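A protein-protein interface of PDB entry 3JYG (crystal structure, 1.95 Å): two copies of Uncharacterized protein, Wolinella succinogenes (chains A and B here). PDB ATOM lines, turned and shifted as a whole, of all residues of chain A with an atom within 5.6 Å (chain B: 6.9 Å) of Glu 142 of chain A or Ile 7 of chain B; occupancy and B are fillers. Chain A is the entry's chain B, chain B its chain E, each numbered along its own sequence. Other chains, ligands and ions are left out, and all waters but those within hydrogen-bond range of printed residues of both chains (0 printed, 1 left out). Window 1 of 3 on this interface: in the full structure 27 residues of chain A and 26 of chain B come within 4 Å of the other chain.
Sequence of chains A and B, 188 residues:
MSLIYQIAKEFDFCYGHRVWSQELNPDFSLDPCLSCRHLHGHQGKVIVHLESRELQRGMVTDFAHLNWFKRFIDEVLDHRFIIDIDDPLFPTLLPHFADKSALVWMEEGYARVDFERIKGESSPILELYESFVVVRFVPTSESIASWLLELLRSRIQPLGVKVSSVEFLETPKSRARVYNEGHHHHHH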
ATOM      1  N   THR A 140     -24.743  -9.265  36.990  1.00  0.00           N
ATOM      2  CA  THR A 140     -23.956 -10.127  36.120  1.00  0.00           C
ATOM      3  C   THR A 140     -22.492  -9.691  36.307  1.00  0.00           C
ATOM      4  O   THR A 140     -22.228  -8.608  36.834  1.00  0.00           O
ATOM      5  CB  THR A 140     -24.394  -9.980  34.621  1.00  0.00           C
ATOM      6  OG1 THR A 140     -24.313  -8.601  34.234  1.00  0.00           O
ATOM      7  CG2 THR A 140     -25.834 -10.453  34.416  1.00  0.00           C
ATOM      8  N   SER A 141     -21.553 -10.509  35.829  1.00  0.00           N
ATOM      9  CA  SER A 141     -20.147 -10.112  35.778  1.00  0.00           C
ATOM     10  C   SER A 141     -19.947  -8.840  35.013  1.00  0.00           C
ATOM     11  O   SER A 141     -19.191  -8.020  35.456  1.00  0.00           O
ATOM     12  CB  SER A 141     -19.289 -11.194  35.140  1.00  0.00           C
ATOM     13  OG  SER A 141     -19.459 -12.454  35.776  1.00  0.00           O
ATOM     14  N   GLU A 142     -20.613  -8.681  33.854  1.00  0.00           N
ATOM     15  CA  GLU A 142     -20.479  -7.450  33.066  1.00  0.00           C
ATOM     16  C   GLU A 142     -20.988  -6.229  33.832  1.00  0.00           C
ATOM     17  O   GLU A 142     -20.397  -5.109  33.782  1.00  0.00           O
ATOM     18  CB  GLU A 142     -21.261  -7.562  31.776  1.00  0.00           C
ATOM     19  CG  GLU A 142     -20.742  -8.595  30.790  1.00  0.00           C
ATOM     20  CD  GLU A 142     -21.476  -9.922  30.905  1.00  0.00           C
ATOM     21  OE1 GLU A 142     -21.669 -10.447  32.051  1.00  0.00           O
ATOM     22  OE2 GLU A 142     -21.873 -10.440  29.843  1.00  0.00           O
ATOM     23  N   SER A 143     -22.102  -6.417  34.509  1.00  0.00           N
ATOM     24  CA  SER A 143     -22.659  -5.318  35.315  1.00  0.00           C
ATOM     25  C   SER A 143     -21.816  -4.917  36.489  1.00  0.00           C
ATOM     26  O   SER A 143     -21.637  -3.708  36.761  1.00  0.00           O
ATOM     27  CB  SER A 143     -24.075  -5.665  35.782  1.00  0.00           C
ATOM     28  OG  SER A 143     -24.922  -5.507  34.679  1.00  0.00           O
ATOM     29  N   ILE A 144     -21.356  -5.912  37.248  1.00  0.00           N
ATOM     30  CA  ILE A 144     -20.507  -5.614  38.348  1.00  0.00           C
ATOM     31  C   ILE A 144     -19.239  -4.861  37.898  1.00  0.00           C
ATOM     32  O   ILE A 144     -18.829  -3.872  38.536  1.00  0.00           O
ATOM     33  CB  ILE A 144     -20.153  -6.902  39.134  1.00  0.00           C
ATOM     34  CG1 ILE A 144     -21.406  -7.338  39.915  1.00  0.00           C
ATOM     35  CG2 ILE A 144     -18.975  -6.619  40.085  1.00  0.00           C
ATOM     36  CD1 ILE A 144     -21.397  -8.832  40.422  1.00  0.00           C
ATOM     37  N   ALA A 145     -18.632  -5.337  36.806  1.00  0.00           N
ATOM     38  CA  ALA A 145     -17.417  -4.773  36.265  1.00  0.00           C
ATOM     39  C   ALA A 145     -17.645  -3.300  35.864  1.00  0.00           C
ATOM     40  O   ALA A 145     -16.823  -2.444  36.184  1.00  0.00           O
ATOM     41  CB  ALA A 145     -16.923  -5.619  35.087  1.00  0.00           C
ATOM     42  N   SER A 146     -18.767  -3.021  35.201  1.00  0.00           N
ATOM     43  CA  SER A 146     -19.145  -1.623  34.806  1.00  0.00           C
ATOM     44  C   SER A 146     -19.296  -0.746  36.023  1.00  0.00           C
ATOM     45  O   SER A 146     -18.833   0.399  36.022  1.00  0.00           O
ATOM     46  CB  SER A 146     -20.473  -1.601  34.020  1.00  0.00           C
ATOM     47  OG  SER A 146     -20.412  -2.467  32.888  1.00  0.00           O
ATOM     48  N   TRP A 147     -19.895  -1.278  37.072  1.00  0.00           N
ATOM     49  CA  TRP A 147     -20.114  -0.491  38.313  1.00  0.00           C
ATOM     50  C   TRP A 147     -18.823  -0.188  39.004  1.00  0.00           C
ATOM     51  O   TRP A 147     -18.613   0.951  39.462  1.00  0.00           O
ATOM     52  CB  TRP A 147     -21.024  -1.265  39.243  1.00  0.00           C
ATOM     53  CG  TRP A 147     -21.275  -0.674  40.564  1.00  0.00           C
ATOM     54  CD1 TRP A 147     -21.692   0.602  40.844  1.00  0.00           C
ATOM     55  CD2 TRP A 147     -21.168  -1.347  41.816  1.00  0.00           C
ATOM     56  NE1 TRP A 147     -21.830   0.768  42.196  1.00  0.00           N
ATOM     57  CE2 TRP A 147     -21.531  -0.419  42.817  1.00  0.00           C
ATOM     58  CE3 TRP A 147     -20.806  -2.658  42.189  1.00  0.00           C
ATOM     59  CZ2 TRP A 147     -21.551  -0.757  44.180  1.00  0.00           C
ATOM     60  CZ3 TRP A 147     -20.806  -2.983  43.535  1.00  0.00           C
ATOM     61  CH2 TRP A 147     -21.169  -2.029  44.515  1.00  0.00           C
ATOM     62  N   ARG A 175     -15.080 -14.754  32.435  1.00  0.00           N
ATOM     63  CA  ARG A 175     -14.869 -13.404  32.937  1.00  0.00           C
ATOM     64  C   ARG A 175     -15.418 -12.357  32.005  1.00  0.00           C
ATOM     65  O   ARG A 175     -15.682 -12.617  30.845  1.00  0.00           O
ATOM     66  CB  ARG A 175     -13.383 -13.134  33.253  1.00  0.00           C
ATOM     67  CG  ARG A 175     -12.360 -13.380  32.103  1.00  0.00           C
ATOM     68  CD  ARG A 175     -11.027 -13.830  32.727  1.00  0.00           C
ATOM     69  NE  ARG A 175     -10.012 -14.244  31.761  1.00  0.00           N
ATOM     70  CZ  ARG A 175     -10.165 -15.238  30.887  1.00  0.00           C
ATOM     71  NH1 ARG A 175     -11.312 -15.917  30.835  1.00  0.00           N
ATOM     72  NH2 ARG A 175      -9.176 -15.545  30.068  1.00  0.00           N
ATOM     73  N   ALA A 176     -15.583 -11.167  32.548  1.00  0.00           N
ATOM     74  CA  ALA A 176     -16.084 -10.024  31.824  1.00  0.00           C
ATOM     75  C   ALA A 176     -14.988  -8.971  31.839  1.00  0.00           C
ATOM     76  O   ALA A 176     -14.158  -8.955  32.720  1.00  0.00           O
ATOM     77  CB  ALA A 176     -17.379  -9.506  32.516  1.00  0.00           C
ATOM     78  N   ARG A 177     -14.970  -8.094  30.854  1.00  0.00           N
ATOM     79  CA  ARG A 177     -14.054  -6.969  30.875  1.00  0.00           C
ATOM     80  C   ARG A 177     -14.811  -5.756  30.302  1.00  0.00           C
ATOM     81  O   ARG A 177     -15.529  -5.868  29.308  1.00  0.00           O
ATOM     82  CB  ARG A 177     -12.826  -7.282  30.014  1.00  0.00           C
ATOM     83  CG  ARG A 177     -11.757  -6.184  29.954  1.00  0.00           C
ATOM     84  CD  ARG A 177     -10.394  -6.762  29.581  1.00  0.00           C
ATOM     85  NE  ARG A 177      -9.274  -5.893  29.933  1.00  0.00           N
ATOM     86  CZ  ARG A 177      -8.005  -6.274  29.826  1.00  0.00           C
ATOM     87  NH1 ARG A 177      -7.735  -7.501  29.390  1.00  0.00           N
ATOM     88  NH2 ARG A 177      -7.003  -5.450  30.141  1.00  0.00           N
ATOM     89  N   VAL A 178     -14.655  -4.612  30.943  1.00  0.00           N
ATOM     90  CA  VAL A 178     -15.173  -3.390  30.408  1.00  0.00           C
ATOM     91  C   VAL A 178     -14.019  -2.413  30.196  1.00  0.00           C
ATOM     92  O   VAL A 178     -13.315  -2.072  31.150  1.00  0.00           O
ATOM     93  CB  VAL A 178     -16.276  -2.759  31.313  1.00  0.00           C
ATOM     94  CG1 VAL A 178     -16.956  -1.576  30.570  1.00  0.00           C
ATOM     95  CG2 VAL A 178     -17.346  -3.816  31.725  1.00  0.00           C
ATOM     96  N   TYR B   5     -17.577  -3.680  25.764  1.00  0.00           N
ATOM     97  CA  TYR B   5     -17.810  -4.828  26.677  1.00  0.00           C
ATOM     98  C   TYR B   5     -17.363  -6.143  26.095  1.00  0.00           C
ATOM     99  O   TYR B   5     -17.718  -6.448  24.959  1.00  0.00           O
ATOM    100  CB  TYR B   5     -19.277  -4.946  27.087  1.00  0.00           C
ATOM    101  CG  TYR B   5     -19.896  -3.612  27.494  1.00  0.00           C
ATOM    102  CD1 TYR B   5     -20.555  -2.815  26.534  1.00  0.00           C
ATOM    103  CD2 TYR B   5     -19.816  -3.130  28.837  1.00  0.00           C
ATOM    104  CE1 TYR B   5     -21.121  -1.574  26.905  1.00  0.00           C
ATOM    105  CE2 TYR B   5     -20.406  -1.867  29.198  1.00  0.00           C
ATOM    106  CZ  TYR B   5     -21.046  -1.114  28.211  1.00  0.00           C
ATOM    107  OH  TYR B   5     -21.657   0.118  28.435  1.00  0.00           O
ATOM    108  N   GLN B   6     -16.643  -6.933  26.897  1.00  0.00           N
ATOM    109  CA  GLN B   6     -16.194  -8.190  26.449  1.00  0.00           C
ATOM    110  C   GLN B   6     -16.448  -9.258  27.511  1.00  0.00           C
ATOM    111  O   GLN B   6     -16.488  -8.981  28.716  1.00  0.00           O
ATOM    112  CB  GLN B   6     -14.707  -8.156  26.115  1.00  0.00           C
ATOM    113  CG  GLN B   6     -14.337  -7.328  24.849  1.00  0.00           C
ATOM    114  CD  GLN B   6     -12.832  -7.392  24.494  1.00  0.00           C
ATOM    115  OE1 GLN B   6     -12.013  -7.919  25.258  1.00  0.00           O
ATOM    116  NE2 GLN B   6     -12.483  -6.841  23.344  1.00  0.00           N
ATOM    117  N   ILE B   7     -16.607 -10.481  27.048  1.00  0.00           N
ATOM    118  CA  ILE B   7     -16.532 -11.584  27.974  1.00  0.00           C
ATOM    119  C   ILE B   7     -15.546 -12.531  27.328  1.00  0.00           C
ATOM    120  O   ILE B   7     -15.320 -12.452  26.091  1.00  0.00           O
ATOM    121  CB  ILE B   7     -17.895 -12.250  28.206  1.00  0.00           C
ATOM    122  CG1 ILE B   7     -18.482 -12.788  26.894  1.00  0.00           C
ATOM    123  CG2 ILE B   7     -18.889 -11.260  28.928  1.00  0.00           C
ATOM    124  CD1 ILE B   7     -19.582 -13.822  27.081  1.00  0.00           C
ATOM    125  N   ALA B   8     -14.965 -13.405  28.146  1.00  0.00           N
ATOM    126  CA  ALA B   8     -14.037 -14.445  27.652  1.00  0.00           C
ATOM    127  C   ALA B   8     -14.356 -15.737  28.379  1.00  0.00           C
ATOM    128  O   ALA B   8     -14.641 -15.700  29.569  1.00  0.00           O
ATOM    129  CB  ALA B   8     -12.618 -14.067  27.921  1.00  0.00           C
ATOM    130  N   LYS B   9     -14.269 -16.873  27.693  1.00  0.00           N
ATOM    131  CA  LYS B   9     -14.482 -18.175  28.369  1.00  0.00           C
ATOM    132  C   LYS B   9     -13.427 -19.166  27.840  1.00  0.00           C
ATOM    133  O   LYS B   9     -13.072 -19.122  26.647  1.00  0.00           O
ATOM    134  CB  LYS B   9     -15.904 -18.703  28.115  1.00  0.00           C
ATOM    135  CG  LYS B   9     -16.086 -20.076  28.793  1.00  0.00           C
ATOM    136  CD  LYS B   9     -17.466 -20.400  29.229  1.00  0.00           C
ATOM    137  CE  LYS B   9     -17.472 -21.808  29.836  1.00  0.00           C
ATOM    138  NZ  LYS B   9     -18.913 -22.276  29.940  1.00  0.00           N
ATOM    139  N   VAL B  48     -12.021 -17.903  24.250  1.00  0.00           N
ATOM    140  CA  VAL B  48     -12.869 -17.195  23.266  1.00  0.00           C
ATOM    141  C   VAL B  48     -13.245 -15.823  23.901  1.00  0.00           C
ATOM    142  O   VAL B  48     -13.809 -15.770  25.011  1.00  0.00           O
ATOM    143  CB  VAL B  48     -14.159 -18.030  22.914  1.00  0.00           C
ATOM    144  CG1 VAL B  48     -15.029 -17.302  21.929  1.00  0.00           C
ATOM    145  CG2 VAL B  48     -13.795 -19.448  22.344  1.00  0.00           C
ATOM    146  N   HIS B  49     -12.892 -14.732  23.213  1.00  0.00           N
ATOM    147  CA  HIS B  49     -13.343 -13.381  23.573  1.00  0.00           C
ATOM    148  C   HIS B  49     -14.441 -12.900  22.642  1.00  0.00           C
ATOM    149  O   HIS B  49     -14.274 -12.886  21.373  1.00  0.00           O
ATOM    150  CB  HIS B  49     -12.171 -12.399  23.545  1.00  0.00           C
ATOM    151  CG  HIS B  49     -11.011 -12.857  24.351  1.00  0.00           C
ATOM    152  ND1 HIS B  49     -10.666 -12.279  25.557  1.00  0.00           N
ATOM    153  CD2 HIS B  49     -10.103 -13.832  24.120  1.00  0.00           C
ATOM    154  CE1 HIS B  49      -9.609 -12.906  26.051  1.00  0.00           C
ATOM    155  NE2 HIS B  49      -9.245 -13.849  25.193  1.00  0.00           N
ATOM    156  N   LEU B  50     -15.563 -12.536  23.272  1.00  0.00           N
ATOM    157  CA  LEU B  50     -16.742 -11.971  22.539  1.00  0.00           C
ATOM    158  C   LEU B  50     -16.953 -10.514  22.973  1.00  0.00           C
ATOM    159  O   LEU B  50     -16.713 -10.197  24.109  1.00  0.00           O
ATOM    160  CB  LEU B  50     -18.001 -12.744  22.847  1.00  0.00           C
ATOM    161  CG  LEU B  50     -17.897 -14.249  22.568  1.00  0.00           C
ATOM    162  CD1 LEU B  50     -19.183 -14.936  22.951  1.00  0.00           C
ATOM    163  CD2 LEU B  50     -17.589 -14.536  21.081  1.00  0.00           C
ATOM    164  N   GLU B  51     -17.398  -9.653  22.056  1.00  0.00           N
ATOM    165  CA  GLU B  51     -17.482  -8.217  22.316  1.00  0.00           C
ATOM    166  C   GLU B  51     -18.833  -7.675  21.831  1.00  0.00           C
ATOM    167  O   GLU B  51     -19.405  -8.155  20.849  1.00  0.00           O
ATOM    168  CB  GLU B  51     -16.301  -7.521  21.622  1.00  0.00           C
ATOM    169  CG  GLU B  51     -16.342  -6.027  21.521  1.00  0.00           C
ATOM    170  CD  GLU B  51     -15.054  -5.478  20.912  1.00  0.00           C
ATOM    171  OE1 GLU B  51     -13.958  -5.716  21.466  1.00  0.00           O
ATOM    172  OE2 GLU B  51     -15.153  -4.803  19.872  1.00  0.00           O
ATOM    173  N   SER B  52     -19.361  -6.708  22.545  1.00  0.00           N
ATOM    174  CA  SER B  52     -20.544  -5.994  22.095  1.00  0.00           C
ATOM    175  C   SER B  52     -20.393  -4.545  22.489  1.00  0.00           C
ATOM    176  O   SER B  52     -19.669  -4.209  23.437  1.00  0.00           O
ATOM    177  CB  SER B  52     -21.802  -6.548  22.732  1.00  0.00           C
ATOM    178  OG  SER B  52     -21.626  -6.481  24.138  1.00  0.00           O
ATOM    179  N   LEU B  55     -24.726  -3.680  26.504  1.00  0.00           N
ATOM    180  CA  LEU B  55     -25.225  -4.847  27.281  1.00  0.00           C
ATOM    181  C   LEU B  55     -26.717  -5.028  27.039  1.00  0.00           C
ATOM    182  O   LEU B  55     -27.438  -4.031  26.824  1.00  0.00           O
ATOM    183  CB  LEU B  55     -24.928  -4.700  28.792  1.00  0.00           C
ATOM    184  CG  LEU B  55     -23.479  -4.491  29.270  1.00  0.00           C
ATOM    185  CD1 LEU B  55     -23.412  -4.301  30.805  1.00  0.00           C
ATOM    186  CD2 LEU B  55     -22.660  -5.675  28.848  1.00  0.00           C
ATOM    187  N   GLN B  56     -27.170  -6.275  27.026  1.00  0.00           N
ATOM    188  CA  GLN B  56     -28.582  -6.605  26.957  1.00  0.00           C
ATOM    189  C   GLN B  56     -28.892  -7.510  28.126  1.00  0.00           C
ATOM    190  O   GLN B  56     -28.236  -8.552  28.277  1.00  0.00           O
ATOM    191  CB  GLN B  56     -28.931  -7.311  25.637  1.00  0.00           C
ATOM    192  CG  GLN B  56     -29.164  -6.231  24.534  1.00  0.00           C
ATOM    193  CD  GLN B  56     -29.513  -6.809  23.169  1.00  0.00           C
ATOM    194  OE1 GLN B  56     -28.874  -7.765  22.696  1.00  0.00           O
ATOM    195  NE2 GLN B  56     -30.498  -6.203  22.511  1.00  0.00           N
ATOM    196  N   GLY B  58     -27.972  -6.982  30.976  1.00  0.00           N
ATOM    197  CA  GLY B  58     -26.719  -7.014  31.744  1.00  0.00           C
ATOM    198  C   GLY B  58     -25.543  -7.793  31.173  1.00  0.00           C
ATOM    199  O   GLY B  58     -24.553  -7.943  31.834  1.00  0.00           O
ATOM    200  N   MET B  59     -25.621  -8.222  29.916  1.00  0.00           N
ATOM    201  CA  MET B  59     -24.663  -9.172  29.391  1.00  0.00           C
ATOM    202  C   MET B  59     -24.212  -8.783  27.968  1.00  0.00           C
ATOM    203  O   MET B  59     -24.958  -8.145  27.209  1.00  0.00           O
ATOM    204  CB  MET B  59     -25.322 -10.542  29.306  1.00  0.00           C
ATOM    205  CG  MET B  59     -25.603 -11.280  30.612  1.00  0.00           C
ATOM    206  SD  MET B  59     -26.337 -13.020  30.160  1.00  0.00           S
ATOM    207  CE  MET B  59     -27.126 -13.323  31.908  1.00  0.00           C
ATOM    208  N   VAL B  60     -22.994  -9.203  27.618  1.00  0.00           N
ATOM    209  CA  VAL B  60     -22.552  -9.219  26.247  1.00  0.00           C
ATOM    210  C   VAL B  60     -23.471 -10.257  25.575  1.00  0.00           C
ATOM    211  O   VAL B  60     -24.241  -9.924  24.687  1.00  0.00           O
ATOM    212  CB  VAL B  60     -21.088  -9.584  26.163  1.00  0.00           C
ATOM    213  CG1 VAL B  60     -20.663  -9.889  24.734  1.00  0.00           C
ATOM    214  CG2 VAL B  60     -20.234  -8.412  26.756  1.00  0.00           C
ATOM    215  N   THR B  61     -23.389 -11.498  26.054  1.00  0.00           N
ATOM    216  CA  THR B  61     -24.303 -12.586  25.719  1.00  0.00           C
ATOM    217  C   THR B  61     -23.980 -13.612  26.802  1.00  0.00           C
ATOM    218  O   THR B  61     -22.898 -13.538  27.418  1.00  0.00           O
ATOM    219  CB  THR B  61     -24.043 -13.219  24.337  1.00  0.00           C
ATOM    220  OG1 THR B  61     -25.155 -14.042  24.004  1.00  0.00           O
ATOM    221  CG2 THR B  61     -22.813 -14.109  24.342  1.00  0.00           C
ATOM    222  N   ASP B  62     -24.890 -14.536  27.034  1.00  0.00           N
ATOM    223  CA  ASP B  62     -24.712 -15.518  28.143  1.00  0.00           C
ATOM    224  C   ASP B  62     -23.529 -16.471  27.866  1.00  0.00           C
ATOM    225  O   ASP B  62     -23.440 -17.054  26.762  1.00  0.00           O
ATOM    226  CB  ASP B  62     -25.958 -16.390  28.319  1.00  0.00           C
ATOM    227  CG  ASP B  62     -26.034 -17.007  29.699  1.00  0.00           C
ATOM    228  OD1 ASP B  62     -25.266 -17.977  29.994  1.00  0.00           O
ATOM    229  OD2 ASP B  62     -26.871 -16.517  30.491  1.00  0.00           O
ATOM    230  N   PHE B  63     -22.645 -16.633  28.863  1.00  0.00           N
ATOM    231  CA  PHE B  63     -21.601 -17.674  28.818  1.00  0.00           C
ATOM    232  C   PHE B  63     -22.083 -19.014  28.258  1.00  0.00           C
ATOM    233  O   PHE B  63     -21.309 -19.705  27.550  1.00  0.00           O
ATOM    234  CB  PHE B  63     -20.957 -17.879  30.211  1.00  0.00           C
ATOM    235  CG  PHE B  63     -20.114 -16.709  30.675  1.00  0.00           C
ATOM    236  CD1 PHE B  63     -18.999 -16.296  29.936  1.00  0.00           C
ATOM    237  CD2 PHE B  63     -20.426 -16.027  31.872  1.00  0.00           C
ATOM    238  CE1 PHE B  63     -18.205 -15.211  30.369  1.00  0.00           C
ATOM    239  CE2 PHE B  63     -19.642 -14.944  32.310  1.00  0.00           C
ATOM    240  CZ  PHE B  63     -18.526 -14.544  31.548  1.00  0.00           C
ATOM    241  N   ALA B  64     -23.343 -19.376  28.530  1.00  0.00           N
ATOM    242  CA  ALA B  64     -23.909 -20.675  28.068  1.00  0.00           C
ATOM    243  C   ALA B  64     -24.119 -20.755  26.579  1.00  0.00           C
ATOM    244  O   ALA B  64     -24.270 -21.841  26.032  1.00  0.00           O
ATOM    245  CB  ALA B  64     -25.235 -21.037  28.803  1.00  0.00           C
ATOM    246  N   LEU B  66     -21.945 -20.494  24.399  1.00  0.00           N
ATOM    247  CA  LEU B  66     -20.809 -21.230  23.834  1.00  0.00           C
ATOM    248  C   LEU B  66     -20.866 -22.723  24.144  1.00  0.00           C
ATOM    249  O   LEU B  66     -19.903 -23.452  23.831  1.00  0.00           O
ATOM    250  CB  LEU B  66     -19.489 -20.666  24.347  1.00  0.00           C
ATOM    251  CG  LEU B  66     -19.120 -19.316  23.699  1.00  0.00           C
ATOM    252  CD1 LEU B  66     -18.061 -18.504  24.498  1.00  0.00           C
ATOM    253  CD2 LEU B  66     -18.710 -19.504  22.207  1.00  0.00           C
ATOM    254  N   SER B 164     -14.063 -11.130  19.056  1.00  0.00           N
ATOM    255  CA  SER B 164     -12.985 -10.182  18.953  1.00  0.00           C
ATOM    256  C   SER B 164     -11.595 -10.844  18.807  1.00  0.00           C
ATOM    257  O   SER B 164     -10.731 -10.325  18.104  1.00  0.00           O
ATOM    258  CB  SER B 164     -12.999  -9.233  20.135  1.00  0.00           C
ATOM    259  OG  SER B 164     -13.100  -9.990  21.316  1.00  0.00           O
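The backbone carbonyl oxygen of Gly 58 of chain B lies within hydrogen-bond range of the side-chain hydroxyl of Thr 140 of chain A, 2.5 Å away.
The side-chain carboxylate (OE2) of Glu 142 of chain A sits at hydrogen-bond distance from the backbone NH (N) of Val 60 of chain B, 2.8 Å away.
N of Ala 8 of chain B lies within hydrogen-bond range of O of Arg 175 of chain A.
The backbone carbonyl oxygen of Gln 6 of chain B lies within hydrogen-bond range of the backbone NH of Arg 177 of chain A (2.8 Å).
The backbone NH (N) of Ser 143 of chain A lies within hydrogen-bond range of the side-chain hydroxyl (OG1) of Thr 140 of chain A (3.1 Å).
O of Glu 142 of chain A lies within hydrogen-bond range of OG of Ser 146 of chain A, at 2.8 Å.
The backbone carbonyl oxygen (O) of Tyr 5 of chain B sits at hydrogen-bond distance from the backbone NH (N) of Ser 52 of chain B (2.9 Å).
The side-chain amide nitrogen (NE2) of Gln 6 of chain B lies within hydrogen-bond range of the side-chain carboxylate (OE1) of Glu 51 of chain B (2.6 Å).
O of Ile 7 of chain B sits at hydrogen-bond distance from N of Leu 50 of chain B (2.8 Å).
The side-chain sulfur of Met 59 of chain B lies close to the backbone NH of Asp 62 of chain B (3.8 Å).
Among the printed residues, pairs that only touch across the chains: Thr 140 of chain A with Met 59 of chain B (3.9 Å), Glu 142 of chain A with Ile 7 of chain B (3.2 Å), Glu 142 of chain A with Leu 55 of chain B (3.8 Å), Glu 142 of chain A with Gly 58 of chain B (3.3 Å), Glu 142 of chain A with Met 59 of chain B (3.1 Å), Ser 143 of chain A with Gly 58 of chain B (3.8 Å), Ser 146 of chain A with Tyr 5 of chain B (3.7 Å), Arg 175 of chain A with Ile 7 of chain B (3.2 Å), Arg 175 of chain A with Phe 63 of chain B (3.5 Å), Ala 176 of chain A with Gln 6 of chain B (3.3 Å), Arg 177 of chain A with Tyr 5 of chain B (3.6 Å) and Val 178 of chain A with Tyr 5 of chain B (3.7 Å).
Of the printed residues of chain B, Thr 140 of chain A touches Gly 58 (2.5 Å) and Met 59 (3.9 Å).
Of the printed residues of chain B, Glu 142 of chain A touches Ile 7, Leu 55, Gly 58, Met 59 and Val 60.
Of the printed residues of chain B, Val 178 of chain A touches Tyr 5.
Printed residues of chain A within 4 Å of Ile 7 of chain B: Glu 142 and Arg 175.
Of the printed residues of chain A, Met 59 of chain B touches Thr 140 (3.9 Å) and Glu 142 (3.1 Å).
Ala 64 of chain B touches none of the printed residues of chain A.
The nearest printed residue of chain B that does not touch Ser 143 of chain A is Leu 55 of chain B (4.3 Å).
Of the 21 printed residues of chain B, 9 touch a printed residue of chain A.
Printed residues of chain B that touch a printed residue of chain A: Tyr 5, Gln 6, Ile 7, Ala 8, Leu 55, Gly 58, Met 59, Val 60 and Phe 63.
Hydrophobic or aromatic side chains of chain B that line the printed part of chain A: Tyr 5, Ile 7, Ala 8, Leu 55, Met 59, Val 60 and Phe 63.
Of the 12 printed residues of chain A, 8 touch a printed residue of chain B.
Hydrophobic or aromatic side chains of chain A that line the printed part of chain B: Ala 176 and Val 178.
Among the printed residues, 16 pairs touch across the chains.
Among the printed residues, no Asp or Glu carboxylate lies within 4 Å of a Lys or Arg side-chain nitrogen of the other chain.
No position is printed for both chains.
Of the 16 pairs that touch across the chains among the printed residues, none has its exchanged pair printed and touching as well.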
